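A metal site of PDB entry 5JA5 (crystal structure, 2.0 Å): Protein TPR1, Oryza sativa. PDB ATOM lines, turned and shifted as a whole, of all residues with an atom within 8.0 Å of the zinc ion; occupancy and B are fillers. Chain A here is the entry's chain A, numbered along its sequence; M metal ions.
The side-chain sulfur of Cys 204 lies close to the backbone NH of Arg 190 (3.6 Å).
The backbone NH (N) of His 202 lies within hydrogen-bond range of the side-chain amide oxygen (OE1) of Gln 182.
The side-chain sulfur (SG) of Cys 186 sits close to the backbone carbonyl oxygen (O) of Gln 182.
Four residues have an atom within 4 Å of the zinc ion: His 183, Cys 186, His 202 and Cys 204.
The nearest printed residue that does not touch the zinc ion is Thr 203 (4.5 Å).
The zinc ion is bound by a ring nitrogen (NE2) of His 202 (2.4 Å), the side-chain sulfur (SG) of Cys 186 (2.5 Å), a ring nitrogen (ND1) of His 183 (2.5 Å) and the side-chain sulfur (SG) of Cys 204 (2.7 Å).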
ATOM      1  N   LEU A 179      25.360 -11.218  -8.675  1.00  0.00           N
ATOM      2  CA  LEU A 179      26.374 -10.287  -9.160  1.00  0.00           C
ATOM      3  C   LEU A 179      26.386 -10.216 -10.676  1.00  0.00           C
ATOM      4  O   LEU A 179      26.672  -9.161 -11.261  1.00  0.00           O
ATOM      5  CB  LEU A 179      27.757 -10.684  -8.638  1.00  0.00           C
ATOM      6  CG  LEU A 179      27.932 -10.636  -7.112  1.00  0.00           C
ATOM      7  CD1 LEU A 179      29.362 -10.994  -6.700  1.00  0.00           C
ATOM      8  CD2 LEU A 179      27.529  -9.264  -6.557  1.00  0.00           C
ATOM      9  N   ASN A 180      26.098 -11.345 -11.321  1.00  0.00           N
ATOM     10  CA  ASN A 180      25.954 -11.384 -12.776  1.00  0.00           C
ATOM     11  C   ASN A 180      24.750 -10.548 -13.201  1.00  0.00           C
ATOM     12  O   ASN A 180      24.809  -9.812 -14.178  1.00  0.00           O
ATOM     13  CB  ASN A 180      25.806 -12.825 -13.280  1.00  0.00           C
ATOM     14  CG  ASN A 180      27.151 -13.514 -13.471  1.00  0.00           C
ATOM     15  OD1 ASN A 180      27.964 -13.577 -12.554  1.00  0.00           O
ATOM     16  ND2 ASN A 180      27.381 -14.020 -14.671  1.00  0.00           N
ATOM     17  N   TRP A 181      23.658 -10.673 -12.455  1.00  0.00           N
ATOM     18  CA  TRP A 181      22.448  -9.914 -12.755  1.00  0.00           C
ATOM     19  C   TRP A 181      22.678  -8.405 -12.620  1.00  0.00           C
ATOM     20  O   TRP A 181      22.213  -7.630 -13.454  1.00  0.00           O
ATOM     21  CB  TRP A 181      21.299 -10.354 -11.843  1.00  0.00           C
ATOM     22  CG  TRP A 181      19.977  -9.740 -12.193  1.00  0.00           C
ATOM     23  CD1 TRP A 181      19.093 -10.186 -13.136  1.00  0.00           C
ATOM     24  CD2 TRP A 181      19.380  -8.574 -11.600  1.00  0.00           C
ATOM     25  NE1 TRP A 181      17.984  -9.378 -13.161  1.00  0.00           N
ATOM     26  CE2 TRP A 181      18.137  -8.374 -12.230  1.00  0.00           C
ATOM     27  CE3 TRP A 181      19.773  -7.693 -10.590  1.00  0.00           C
ATOM     28  CZ2 TRP A 181      17.289  -7.325 -11.892  1.00  0.00           C
ATOM     29  CZ3 TRP A 181      18.933  -6.642 -10.262  1.00  0.00           C
ATOM     30  CH2 TRP A 181      17.706  -6.479 -10.916  1.00  0.00           C
ATOM     31  N   GLN A 182      23.392  -8.005 -11.584  1.00  0.00           N
ATOM     32  CA  GLN A 182      23.691  -6.589 -11.360  1.00  0.00           C
ATOM     33  C   GLN A 182      24.555  -6.007 -12.476  1.00  0.00           C
ATOM     34  O   GLN A 182      24.281  -4.910 -12.955  1.00  0.00           O
ATOM     35  CB  GLN A 182      24.380  -6.400 -10.016  1.00  0.00           C
ATOM     36  CG  GLN A 182      23.506  -6.732  -8.823  1.00  0.00           C
ATOM     37  CD  GLN A 182      24.284  -6.759  -7.513  1.00  0.00           C
ATOM     38  OE1 GLN A 182      25.370  -6.173  -7.396  1.00  0.00           O
ATOM     39  NE2 GLN A 182      23.735  -7.434  -6.517  1.00  0.00           N
ATOM     40  N   HIS A 183      25.587  -6.740 -12.871  1.00  0.00           N
ATOM     41  CA  HIS A 183      26.505  -6.306 -13.923  1.00  0.00           C
ATOM     42  C   HIS A 183      25.811  -6.239 -15.285  1.00  0.00           C
ATOM     43  O   HIS A 183      26.117  -5.386 -16.112  1.00  0.00           O
ATOM     44  CB  HIS A 183      27.717  -7.250 -13.993  1.00  0.00           C
ATOM     45  CG  HIS A 183      28.613  -6.991 -15.158  1.00  0.00           C
ATOM     46  ND1 HIS A 183      29.370  -5.829 -15.289  1.00  0.00           N
ATOM     47  CD2 HIS A 183      28.910  -7.728 -16.257  1.00  0.00           C
ATOM     48  CE1 HIS A 183      30.062  -5.872 -16.401  1.00  0.00           C
ATOM     49  NE2 HIS A 183      29.808  -7.025 -17.006  1.00  0.00           N
ATOM     50  N   GLN A 184      24.865  -7.145 -15.484  1.00  0.00           N
ATOM     51  CA  GLN A 184      24.122  -7.243 -16.731  1.00  0.00           C
ATOM     52  C   GLN A 184      23.250  -6.006 -16.964  1.00  0.00           C
ATOM     53  O   GLN A 184      22.838  -5.723 -18.098  1.00  0.00           O
ATOM     54  CB  GLN A 184      23.293  -8.543 -16.715  1.00  0.00           C
ATOM     55  CG  GLN A 184      22.136  -8.619 -17.681  1.00  0.00           C
ATOM     56  CD  GLN A 184      20.795  -8.463 -16.976  1.00  0.00           C
ATOM     57  OE1 GLN A 184      20.709  -7.819 -15.932  1.00  0.00           O
ATOM     58  NE2 GLN A 184      19.757  -9.062 -17.535  1.00  0.00           N
ATOM     59  N   LEU A 185      22.989  -5.249 -15.906  1.00  0.00           N
ATOM     60  CA  LEU A 185      22.186  -4.034 -16.008  1.00  0.00           C
ATOM     61  C   LEU A 185      22.994  -2.813 -16.433  1.00  0.00           C
ATOM     62  O   LEU A 185      22.438  -1.772 -16.755  1.00  0.00           O
ATOM     63  CB  LEU A 185      21.503  -3.733 -14.673  1.00  0.00           C
ATOM     64  CG  LEU A 185      20.456  -4.743 -14.196  1.00  0.00           C
ATOM     65  CD1 LEU A 185      19.858  -4.289 -12.868  1.00  0.00           C
ATOM     66  CD2 LEU A 185      19.375  -4.916 -15.242  1.00  0.00           C
ATOM     67  N   CYS A 186      24.324  -2.941 -16.434  1.00  0.00           N
ATOM     68  CA  CYS A 186      25.187  -1.799 -16.669  1.00  0.00           C
ATOM     69  C   CYS A 186      25.393  -1.489 -18.159  1.00  0.00           C
ATOM     70  O   CYS A 186      25.418  -2.387 -18.997  1.00  0.00           O
ATOM     71  CB  CYS A 186      26.537  -2.009 -15.992  1.00  0.00           C
ATOM     72  SG  CYS A 186      26.424  -2.072 -14.188  1.00  0.00           S
ATOM     73  N   LYS A 187      25.534  -0.203 -18.458  1.00  0.00           N
ATOM     74  CA  LYS A 187      25.774   0.276 -19.818  1.00  0.00           C
ATOM     75  C   LYS A 187      26.280   1.722 -19.790  1.00  0.00           C
ATOM     76  O   LYS A 187      25.605   2.597 -19.253  1.00  0.00           O
ATOM     77  CB  LYS A 187      24.511   0.173 -20.662  1.00  0.00           C
ATOM     78  N   ASN A 188      27.461   1.966 -20.355  1.00  0.00           N
ATOM     79  CA  ASN A 188      28.292   0.922 -20.963  1.00  0.00           C
ATOM     80  C   ASN A 188      29.078   0.128 -19.924  1.00  0.00           C
ATOM     81  O   ASN A 188      29.788   0.704 -19.098  1.00  0.00           O
ATOM     82  CB  ASN A 188      29.251   1.553 -21.983  1.00  0.00           C
ATOM     83  N   PRO A 189      28.956  -1.204 -19.978  1.00  0.00           N
ATOM     84  CA  PRO A 189      29.594  -2.062 -18.971  1.00  0.00           C
ATOM     85  C   PRO A 189      31.122  -2.074 -19.100  1.00  0.00           C
ATOM     86  O   PRO A 189      31.659  -2.333 -20.182  1.00  0.00           O
ATOM     87  CB  PRO A 189      29.014  -3.450 -19.256  1.00  0.00           C
ATOM     88  CG  PRO A 189      28.701  -3.416 -20.709  1.00  0.00           C
ATOM     89  CD  PRO A 189      28.252  -2.006 -20.998  1.00  0.00           C
ATOM     90  N   ARG A 190      31.820  -1.794 -18.003  1.00  0.00           N
ATOM     91  CA  ARG A 190      33.279  -1.750 -17.980  1.00  0.00           C
ATOM     92  C   ARG A 190      33.897  -3.122 -18.227  1.00  0.00           C
ATOM     93  O   ARG A 190      34.955  -3.455 -17.664  1.00  0.00           O
ATOM     94  CB  ARG A 190      33.777  -1.202 -16.641  1.00  0.00           C
ATOM     95  N   ILE A 195      33.595  -5.757  -8.857  1.00  0.00           N
ATOM     96  CA  ILE A 195      32.607  -5.695  -7.774  1.00  0.00           C
ATOM     97  C   ILE A 195      33.217  -5.124  -6.506  1.00  0.00           C
ATOM     98  O   ILE A 195      34.239  -5.610  -6.016  1.00  0.00           O
ATOM     99  CB  ILE A 195      32.019  -7.088  -7.460  1.00  0.00           C
ATOM    100  CG1 ILE A 195      31.604  -7.792  -8.751  1.00  0.00           C
ATOM    101  CG2 ILE A 195      30.854  -6.956  -6.502  1.00  0.00           C
ATOM    102  CD1 ILE A 195      30.585  -7.033  -9.571  1.00  0.00           C
ATOM    103  N   HIS A 202      26.195  -3.466  -7.550  1.00  0.00           N
ATOM    104  CA  HIS A 202      27.340  -3.050  -8.342  1.00  0.00           C
ATOM    105  C   HIS A 202      26.891  -2.122  -9.459  1.00  0.00           C
ATOM    106  O   HIS A 202      25.760  -2.224  -9.941  1.00  0.00           O
ATOM    107  CB  HIS A 202      28.057  -4.280  -8.927  1.00  0.00           C
ATOM    108  CG  HIS A 202      28.687  -4.035 -10.261  1.00  0.00           C
ATOM    109  ND1 HIS A 202      29.994  -3.633 -10.396  1.00  0.00           N
ATOM    110  CD2 HIS A 202      28.195  -4.140 -11.511  1.00  0.00           C
ATOM    111  CE1 HIS A 202      30.283  -3.491 -11.684  1.00  0.00           C
ATOM    112  NE2 HIS A 202      29.206  -3.796 -12.382  1.00  0.00           N
ATOM    113  N   THR A 203      27.763  -1.203  -9.866  1.00  0.00           N
ATOM    114  CA  THR A 203      27.462  -0.333 -10.998  1.00  0.00           C
ATOM    115  C   THR A 203      28.694  -0.049 -11.862  1.00  0.00           C
ATOM    116  O   THR A 203      29.815  -0.012 -11.367  1.00  0.00           O
ATOM    117  CB  THR A 203      26.875   1.012 -10.522  1.00  0.00           C
ATOM    118  OG1 THR A 203      26.612   1.849 -11.658  1.00  0.00           O
ATOM    119  CG2 THR A 203      27.828   1.726  -9.582  1.00  0.00           C
ATOM    120  N   CYS A 204      28.448   0.123 -13.157  1.00  0.00           N
ATOM    121  CA  CYS A 204      29.464   0.600 -14.093  1.00  0.00           C
ATOM    122  C   CYS A 204      28.973   1.893 -14.727  1.00  0.00           C
ATOM    123  O   CYS A 204      28.015   1.873 -15.502  1.00  0.00           O
ATOM    124  CB  CYS A 204      29.763  -0.444 -15.179  1.00  0.00           C
ATOM    125  SG  CYS A 204      30.612  -1.942 -14.610  1.00  0.00           S
ATOM    126  N   THR A 205      29.621   3.003 -14.397  1.00  0.00           N
ATOM    127  CA  THR A 205      29.209   4.305 -14.903  1.00  0.00           C
ATOM    128  C   THR A 205      29.352   4.369 -16.427  1.00  0.00           C
ATOM    129  O   THR A 205      28.392   4.107 -17.158  1.00  0.00           O
ATOM    130  CB  THR A 205      30.021   5.463 -14.275  1.00  0.00           C
ATOM    131  OG1 THR A 205      31.251   5.642 -14.991  1.00  0.00           O
ATOM    132  CG2 THR A 205      30.328   5.164 -12.806  1.00  0.00           C
HETATM  133 ZN    ZN M   1      28.406  -3.573 -14.619  1.00  0.00          ZN
